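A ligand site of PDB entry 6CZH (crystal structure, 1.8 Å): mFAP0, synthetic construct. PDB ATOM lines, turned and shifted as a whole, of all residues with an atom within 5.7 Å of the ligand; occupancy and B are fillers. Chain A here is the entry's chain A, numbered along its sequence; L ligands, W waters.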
ATOM      1  N   VAL A  14      18.637   2.010 -16.879  1.00  0.00           N
ATOM      2  CA  VAL A  14      18.406   2.588 -18.206  1.00  0.00           C
ATOM      3  C   VAL A  14      17.932   4.027 -18.069  1.00  0.00           C
ATOM      4  O   VAL A  14      17.065   4.339 -17.253  1.00  0.00           O
ATOM      5  CB  VAL A  14      17.377   1.762 -19.011  1.00  0.00           C
ATOM      6  CG1 VAL A  14      17.228   2.340 -20.411  1.00  0.00           C
ATOM      7  CG2 VAL A  14      17.799   0.301 -19.067  1.00  0.00           C
ATOM      8  N   THR A  15      18.509   4.897 -18.902  1.00  0.00           N
ATOM      9  CA  THR A  15      18.070   6.278 -19.054  1.00  0.00           C
ATOM     10  C   THR A  15      17.849   6.518 -20.539  1.00  0.00           C
ATOM     11  O   THR A  15      18.664   6.107 -21.358  1.00  0.00           O
ATOM     12  CB  THR A  15      19.101   7.273 -18.482  1.00  0.00           C
ATOM     13  OG1 THR A  15      19.444   6.894 -17.143  1.00  0.00           O
ATOM     14  CG2 THR A  15      18.536   8.683 -18.475  1.00  0.00           C
ATOM     15  N   MET A  16      16.748   7.186 -20.876  1.00  0.00           N
ATOM     16  CA  MET A  16      16.393   7.382 -22.270  1.00  0.00           C
ATOM     17  C   MET A  16      15.871   8.798 -22.483  1.00  0.00           C
ATOM     18  O   MET A  16      15.418   9.460 -21.549  1.00  0.00           O
ATOM     19  CB  MET A  16      15.337   6.370 -22.725  1.00  0.00           C
ATOM     20  CG  MET A  16      15.533   4.985 -22.158  1.00  0.00           C
ATOM     21  SD  MET A  16      14.552   3.757 -23.017  1.00  0.00           S
ATOM     22  CE  MET A  16      15.360   3.756 -24.621  1.00  0.00           C
ATOM     23  N   THR A  17      15.944   9.234 -23.738  1.00  0.00           N
ATOM     24  CA  THR A  17      15.374  10.497 -24.181  1.00  0.00           C
ATOM     25  C   THR A  17      14.701  10.256 -25.523  1.00  0.00           C
ATOM     26  O   THR A  17      15.213   9.489 -26.345  1.00  0.00           O
ATOM     27  CB  THR A  17      16.451  11.580 -24.304  1.00  0.00           C
ATOM     28  OG1 THR A  17      17.259  11.595 -23.129  1.00  0.00           O
ATOM     29  CG2 THR A  17      15.813  12.939 -24.483  1.00  0.00           C
ATOM     30  N   ASN A  18      13.556  10.898 -25.749  1.00  0.00           N
ATOM     31  CA  ASN A  18      12.862  10.695 -27.007  1.00  0.00           C
ATOM     32  C   ASN A  18      12.793  12.011 -27.780  1.00  0.00           C
ATOM     33  O   ASN A  18      13.176  13.076 -27.303  1.00  0.00           O
ATOM     34  CB  ASN A  18      11.476  10.079 -26.805  1.00  0.00           C
ATOM     35  CG  ASN A  18      10.512  10.979 -26.048  1.00  0.00           C
ATOM     36  OD1 ASN A  18      10.625  12.203 -26.065  1.00  0.00           O
ATOM     37  ND2 ASN A  18       9.542  10.361 -25.381  1.00  0.00           N
ATOM     38  N   GLN A  22      11.167  14.271 -24.087  1.00  0.00           N
ATOM     39  CA  GLN A  22      10.924  13.649 -22.796  1.00  0.00           C
ATOM     40  C   GLN A  22      12.094  12.747 -22.428  1.00  0.00           C
ATOM     41  O   GLN A  22      12.873  12.321 -23.285  1.00  0.00           O
ATOM     42  CB  GLN A  22       9.619  12.858 -22.833  1.00  0.00           C
ATOM     43  CG  GLN A  22       8.378  13.724 -23.149  1.00  0.00           C
ATOM     44  CD  GLN A  22       7.208  12.917 -23.697  1.00  0.00           C
ATOM     45  OE1 GLN A  22       7.393  11.874 -24.326  1.00  0.00           O
ATOM     46  NE2 GLN A  22       5.989  13.414 -23.482  1.00  0.00           N
ATOM     47  N   THR A  23      12.235  12.485 -21.139  1.00  0.00           N
ATOM     48  CA  THR A  23      13.240  11.558 -20.643  1.00  0.00           C
ATOM     49  C   THR A  23      12.570  10.455 -19.837  1.00  0.00           C
ATOM     50  O   THR A  23      11.441  10.604 -19.382  1.00  0.00           O
ATOM     51  CB  THR A  23      14.289  12.281 -19.782  1.00  0.00           C
ATOM     52  OG1 THR A  23      13.660  12.836 -18.626  1.00  0.00           O
ATOM     53  CG2 THR A  23      14.968  13.385 -20.583  1.00  0.00           C
ATOM     54  N   SER A  24      13.289   9.356 -19.654  1.00  0.00           N
ATOM     55  CA  SER A  24      12.753   8.236 -18.891  1.00  0.00           C
ATOM     56  C   SER A  24      13.887   7.604 -18.087  1.00  0.00           C
ATOM     57  O   SER A  24      15.060   7.706 -18.441  1.00  0.00           O
ATOM     58  CB  SER A  24      12.095   7.189 -19.799  1.00  0.00           C
ATOM     59  OG  SER A  24      13.030   6.622 -20.693  1.00  0.00           O
ATOM     60  N   GLN A  25      13.511   6.967 -16.976  1.00  0.00           N
ATOM     61  CA  GLN A  25      14.451   6.259 -16.116  1.00  0.00           C
ATOM     62  C   GLN A  25      13.811   4.951 -15.672  1.00  0.00           C
ATOM     63  O   GLN A  25      12.607   4.890 -15.436  1.00  0.00           O
ATOM     64  CB  GLN A  25      14.836   7.108 -14.901  1.00  0.00           C
ATOM     65  CG  GLN A  25      15.813   6.423 -13.959  1.00  0.00           C
ATOM     66  N   GLY A  26      14.624   3.897 -15.589  1.00  0.00           N
ATOM     67  CA  GLY A  26      14.085   2.609 -15.167  1.00  0.00           C
ATOM     68  C   GLY A  26      15.109   1.510 -15.343  1.00  0.00           C
ATOM     69  O   GLY A  26      16.321   1.743 -15.272  1.00  0.00           O
ATOM     70  N   GLN A  27      14.592   0.299 -15.569  1.00  0.00           N
ATOM     71  CA  GLN A  27      15.434  -0.874 -15.672  1.00  0.00           C
ATOM     72  C   GLN A  27      14.993  -1.742 -16.843  1.00  0.00           C
ATOM     73  O   GLN A  27      13.839  -1.709 -17.267  1.00  0.00           O
ATOM     74  CB  GLN A  27      15.408  -1.730 -14.401  1.00  0.00           C
ATOM     75  CG  GLN A  27      15.865  -1.009 -13.142  1.00  0.00           C
ATOM     76  CD  GLN A  27      14.792  -0.101 -12.591  1.00  0.00           C
ATOM     77  OE1 GLN A  27      13.606  -0.407 -12.667  1.00  0.00           O
ATOM     78  NE2 GLN A  27      15.206   1.036 -12.046  1.00  0.00           N
ATOM     79  N   MET A  28      15.952  -2.485 -17.375  1.00  0.00           N
ATOM     80  CA  MET A  28      15.675  -3.532 -18.353  1.00  0.00           C
ATOM     81  C   MET A  28      16.305  -4.818 -17.851  1.00  0.00           C
ATOM     82  O   MET A  28      17.402  -4.811 -17.294  1.00  0.00           O
ATOM     83  CB  MET A  28      16.209  -3.185 -19.741  1.00  0.00           C
ATOM     84  CG  MET A  28      15.328  -2.197 -20.509  1.00  0.00           C
ATOM     85  SD  MET A  28      15.979  -1.836 -22.151  1.00  0.00           S
ATOM     86  CE  MET A  28      14.832  -0.575 -22.715  1.00  0.00           C
ATOM     87  N   ALA A  42      10.771  -4.617 -19.148  1.00  0.00           N
ATOM     88  CA  ALA A  42      11.217  -3.259 -18.877  1.00  0.00           C
ATOM     89  C   ALA A  42      10.250  -2.567 -17.926  1.00  0.00           C
ATOM     90  O   ALA A  42       9.031  -2.760 -18.010  1.00  0.00           O
ATOM     91  CB  ALA A  42      11.335  -2.446 -20.173  1.00  0.00           C
ATOM     92  N   GLN A  43      10.805  -1.775 -17.000  1.00  0.00           N
ATOM     93  CA  GLN A  43      10.035  -0.967 -16.066  1.00  0.00           C
ATOM     94  C   GLN A  43      10.659   0.414 -15.973  1.00  0.00           C
ATOM     95  O   GLN A  43      11.878   0.570 -16.087  1.00  0.00           O
ATOM     96  CB  GLN A  43      10.002  -1.572 -14.660  1.00  0.00           C
ATOM     97  CG  GLN A  43       9.087  -2.757 -14.476  1.00  0.00           C
ATOM     98  CD  GLN A  43       8.974  -3.160 -13.009  1.00  0.00           C
ATOM     99  OE1 GLN A  43       9.962  -3.203 -12.278  1.00  0.00           O
ATOM    100  NE2 GLN A  43       7.752  -3.446 -12.570  1.00  0.00           N
ATOM    101  N   GLY A  44       9.821   1.423 -15.715  1.00  0.00           N
ATOM    102  CA  GLY A  44      10.341   2.748 -15.480  1.00  0.00           C
ATOM    103  C   GLY A  44       9.240   3.788 -15.478  1.00  0.00           C
ATOM    104  O   GLY A  44       8.059   3.466 -15.364  1.00  0.00           O
ATOM    105  N   THR A  45       9.657   5.044 -15.634  1.00  0.00           N
ATOM    106  CA  THR A  45       8.741   6.179 -15.651  1.00  0.00           C
ATOM    107  C   THR A  45       9.234   7.216 -16.658  1.00  0.00           C
ATOM    108  O   THR A  45      10.433   7.491 -16.740  1.00  0.00           O
ATOM    109  CB  THR A  45       8.617   6.824 -14.259  1.00  0.00           C
ATOM    110  OG1 THR A  45       8.458   5.812 -13.271  1.00  0.00           O
ATOM    111  CG2 THR A  45       7.413   7.755 -14.227  1.00  0.00           C
ATOM    112  N   ILE A  46       8.305   7.779 -17.421  1.00  0.00           N
ATOM    113  CA  ILE A  46       8.603   8.868 -18.333  1.00  0.00           C
ATOM    114  C   ILE A  46       8.453  10.186 -17.589  1.00  0.00           C
ATOM    115  O   ILE A  46       7.706  10.304 -16.623  1.00  0.00           O
ATOM    116  CB  ILE A  46       7.699   8.805 -19.581  1.00  0.00           C
ATOM    117  CG1 ILE A  46       7.868   7.445 -20.271  1.00  0.00           C
ATOM    118  CG2 ILE A  46       8.028   9.941 -20.556  1.00  0.00           C
ATOM    119  CD1 ILE A  46       6.982   7.255 -21.481  1.00  0.00           C
ATOM    120  N   ARG A  50       4.090   9.170 -17.082  1.00  0.00           N
ATOM    121  CA  ARG A  50       3.541   7.910 -17.576  1.00  0.00           C
ATOM    122  C   ARG A  50       4.377   6.739 -17.088  1.00  0.00           C
ATOM    123  O   ARG A  50       5.603   6.741 -17.254  1.00  0.00           O
ATOM    124  CB  ARG A  50       3.492   7.905 -19.101  1.00  0.00           C
ATOM    125  CG  ARG A  50       2.288   8.587 -19.723  1.00  0.00           C
ATOM    126  CD  ARG A  50       2.360   8.524 -21.241  1.00  0.00           C
ATOM    127  NE  ARG A  50       3.537   9.240 -21.745  1.00  0.00           N
ATOM    128  CZ  ARG A  50       4.084   9.033 -22.931  1.00  0.00           C
ATOM    129  NH1 ARG A  50       3.582   8.124 -23.757  1.00  0.00           N
ATOM    130  NH2 ARG A  50       5.151   9.741 -23.306  1.00  0.00           N
ATOM    131  N   ILE A  52       6.045   3.005 -17.190  1.00  0.00           N
ATOM    132  CA  ILE A  52       6.581   2.158 -18.257  1.00  0.00           C
ATOM    133  C   ILE A  52       6.519   0.705 -17.818  1.00  0.00           C
ATOM    134  O   ILE A  52       7.112   0.328 -16.799  1.00  0.00           O
ATOM    135  CB  ILE A  52       8.026   2.557 -18.609  1.00  0.00           C
ATOM    136  CG1 ILE A  52       8.069   3.982 -19.144  1.00  0.00           C
ATOM    137  CG2 ILE A  52       8.605   1.564 -19.621  1.00  0.00           C
ATOM    138  CD1 ILE A  52       9.474   4.563 -19.203  1.00  0.00           C
ATOM    139  N   ILE A  70      10.017  -4.534 -28.636  1.00  0.00           N
ATOM    140  CA  ILE A  70       9.359  -4.490 -27.332  1.00  0.00           C
ATOM    141  C   ILE A  70       8.031  -3.766 -27.465  1.00  0.00           C
ATOM    142  O   ILE A  70       7.915  -2.790 -28.218  1.00  0.00           O
ATOM    143  CB  ILE A  70      10.273  -3.814 -26.289  1.00  0.00           C
ATOM    144  CG1 ILE A  70       9.554  -3.725 -24.934  1.00  0.00           C
ATOM    145  CG2 ILE A  70      10.698  -2.438 -26.778  1.00  0.00           C
ATOM    146  CD1 ILE A  70      10.504  -3.537 -23.760  1.00  0.00           C
ATOM    147  N   TYR A  72       4.758  -2.020 -25.146  1.00  0.00           N
ATOM    148  CA  TYR A  72       4.514  -1.375 -23.849  1.00  0.00           C
ATOM    149  C   TYR A  72       3.024  -1.283 -23.564  1.00  0.00           C
ATOM    150  O   TYR A  72       2.366  -0.310 -23.951  1.00  0.00           O
ATOM    151  CB  TYR A  72       5.153   0.012 -23.831  1.00  0.00           C
ATOM    152  CG  TYR A  72       6.667  -0.023 -23.922  1.00  0.00           C
ATOM    153  CD1 TYR A  72       7.316   0.062 -25.146  1.00  0.00           C
ATOM    154  CD2 TYR A  72       7.447  -0.144 -22.775  1.00  0.00           C
ATOM    155  CE1 TYR A  72       8.691   0.028 -25.228  1.00  0.00           C
ATOM    156  CE2 TYR A  72       8.827  -0.176 -22.843  1.00  0.00           C
ATOM    157  CZ  TYR A  72       9.449  -0.092 -24.081  1.00  0.00           C
ATOM    158  OH  TYR A  72      10.820  -0.114 -24.156  1.00  0.00           O
ATOM    159  N   LEU A  75       1.756   2.039 -22.167  1.00  0.00           N
ATOM    160  CA  LEU A  75       1.793   3.192 -23.054  1.00  0.00           C
ATOM    161  C   LEU A  75       0.882   2.965 -24.257  1.00  0.00           C
ATOM    162  O   LEU A  75       1.244   3.271 -25.392  1.00  0.00           O
ATOM    163  CB  LEU A  75       3.214   3.492 -23.510  1.00  0.00           C
ATOM    164  CG  LEU A  75       4.286   3.685 -22.424  1.00  0.00           C
ATOM    165  CD1 LEU A  75       5.652   3.878 -23.078  1.00  0.00           C
ATOM    166  CD2 LEU A  75       3.954   4.865 -21.512  1.00  0.00           C
ATOM    167  N   ILE A  78       2.109   0.906 -27.592  1.00  0.00           N
ATOM    168  CA  ILE A  78       3.085   1.351 -28.572  1.00  0.00           C
ATOM    169  C   ILE A  78       4.197   0.318 -28.639  1.00  0.00           C
ATOM    170  O   ILE A  78       4.510  -0.361 -27.647  1.00  0.00           O
ATOM    171  CB  ILE A  78       3.654   2.748 -28.259  1.00  0.00           C
ATOM    172  CG1 ILE A  78       4.688   2.653 -27.149  1.00  0.00           C
ATOM    173  CG2 ILE A  78       2.533   3.709 -27.882  1.00  0.00           C
ATOM    174  CD1 ILE A  78       5.890   3.518 -27.400  1.00  0.00           C
ATOM    175  N   VAL A  80       8.283  -0.591 -29.968  1.00  0.00           N
ATOM    176  CA  VAL A  80       9.600  -0.004 -30.187  1.00  0.00           C
ATOM    177  C   VAL A  80      10.477  -1.043 -30.854  1.00  0.00           C
ATOM    178  O   VAL A  80      10.530  -2.197 -30.413  1.00  0.00           O
ATOM    179  CB  VAL A  80      10.238   0.498 -28.878  1.00  0.00           C
ATOM    180  CG1 VAL A  80      11.653   1.001 -29.131  1.00  0.00           C
ATOM    181  CG2 VAL A  80       9.398   1.597 -28.264  1.00  0.00           C
ATOM    182  N   THR A  98       9.935   4.423 -32.202  1.00  0.00           N
ATOM    183  CA  THR A  98       8.652   3.924 -31.722  1.00  0.00           C
ATOM    184  C   THR A  98       7.685   3.740 -32.883  1.00  0.00           C
ATOM    185  O   THR A  98       7.907   4.224 -33.992  1.00  0.00           O
ATOM    186  CB  THR A  98       8.033   4.871 -30.697  1.00  0.00           C
ATOM    187  OG1 THR A  98       7.513   6.035 -31.367  1.00  0.00           O
ATOM    188  CG2 THR A  98       9.069   5.302 -29.661  1.00  0.00           C
ATOM    189  N   LEU A 104      13.979   7.213 -30.141  1.00  0.00           N
ATOM    190  CA  LEU A 104      14.137   6.892 -28.726  1.00  0.00           C
ATOM    191  C   LEU A 104      15.562   6.412 -28.508  1.00  0.00           C
ATOM    192  O   LEU A 104      15.939   5.366 -29.027  1.00  0.00           O
ATOM    193  CB  LEU A 104      13.125   5.835 -28.289  1.00  0.00           C
ATOM    194  CG  LEU A 104      13.219   5.384 -26.831  1.00  0.00           C
ATOM    195  CD1 LEU A 104      12.911   6.530 -25.877  1.00  0.00           C
ATOM    196  CD2 LEU A 104      12.273   4.213 -26.586  1.00  0.00           C
HETATM  197  F1  LIG L   1      10.335   7.902 -23.277  1.00  0.00           F
HETATM  198  C1  LIG L   1      10.024   6.655 -23.665  1.00  0.00           C
HETATM  199  C2  LIG L   1       9.127   6.479 -24.700  1.00  0.00           C
HETATM  200  O1  LIG L   1       8.568   7.546 -25.310  1.00  0.00           O
HETATM  201  C3  LIG L   1      10.598   5.560 -23.040  1.00  0.00           C
HETATM  202  C4  LIG L   1      10.257   4.264 -23.478  1.00  0.00           C
HETATM  203  C5  LIG L   1       9.339   4.100 -24.515  1.00  0.00           C
HETATM  204  C6  LIG L   1       8.778   5.198 -25.122  1.00  0.00           C
HETATM  205  F2  LIG L   1       7.900   5.037 -26.128  1.00  0.00           F
HETATM  206  C7  LIG L   1      10.782   3.020 -22.902  1.00  0.00           C
HETATM  207  C8  LIG L   1      11.577   2.913 -21.785  1.00  0.00           C
HETATM  208  C9  LIG L   1      12.044   1.610 -21.270  1.00  0.00           C
HETATM  209  O2  LIG L   1      11.794   0.516 -21.742  1.00  0.00           O
HETATM  210  N1  LIG L   1      12.796   1.896 -20.197  1.00  0.00           N
HETATM  211  C10 LIG L   1      13.478   0.907 -19.347  1.00  0.00           C
HETATM  212  C11 LIG L   1      12.813   3.254 -20.030  1.00  0.00           C
HETATM  213  N2  LIG L   1      12.118   3.862 -20.948  1.00  0.00           N
HETATM  214  C12 LIG L   1      13.564   3.936 -18.910  1.00  0.00           C
HETATM  215  O   HOH W   1       6.224   8.074 -25.618  1.00  0.00           O
HETATM  216  O   HOH W   2       8.332   8.791 -27.836  1.00  0.00           O
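The side-chain hydroxyl (OH) of Tyr 72 sits at hydrogen-bond distance from an oxygen (O2) of the ligand (2.7 Å).
OG of Ser 24 lies within hydrogen-bond range of N2 of the ligand (2.9 Å).
An oxygen (O1) of the ligand sits at hydrogen-bond distance from the side-chain amide nitrogen (ND2) of Asn 18, 3.0 Å away.
N of Tyr 72 is in hydrogen-bond range of O of Ile 78.
The backbone carbonyl oxygen (O) of Met 16 sits at hydrogen-bond distance from the backbone NH (N) of Ser 24 (2.9 Å).
ND2 of Asn 18 lies within hydrogen-bond range of OE1 of Gln 22, 2.8 Å away.
N of Ile 52 is in hydrogen-bond range of O of Gly 44, at 2.8 Å.
The backbone carbonyl oxygen (O) of Gln 43 is in hydrogen-bond range of the backbone NH (N) of Gln 27 (2.8 Å).
The backbone carbonyl oxygen (O) of Gln 25 is in hydrogen-bond range of the backbone NH (N) of Thr 45 (3.0 Å).
The backbone carbonyl oxygen (O) of Gly 26 is in hydrogen-bond range of the backbone NH (N) of Val 14 (2.8 Å).
N2 of the ligand lies close to SD of Met 16 (3.2 Å).
Residues that only touch the ligand: Val 14, Gln 25, Gly 26, Gln 27, Met 28, Ala 42, Gln 43, Ile 46, Ile 52, Leu 75, Ile 78, Thr 98 and Leu 104.
Hydrophobic or aromatic side chains that line the ligand: Met 16, Met 28, Ala 42, Ile 46, Ile 52, Tyr 72, Leu 75, Ile 78 and Leu 104.
17 residues have an atom within 4 Å of the ligand: Val 14, Met 16, Asn 18, Ser 24, Gln 25, Gly 26, Gln 27, Met 28, Ala 42, Gln 43, Ile 46, Ile 52, Tyr 72, Leu 75, Ile 78, Thr 98 and Leu 104.
Water W1 bridges an oxygen (O1) of the ligand and the guanidinium group of Arg 50.
Water W2 lies within hydrogen-bond range of O1 of the ligand and ND2 of Asn 18.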
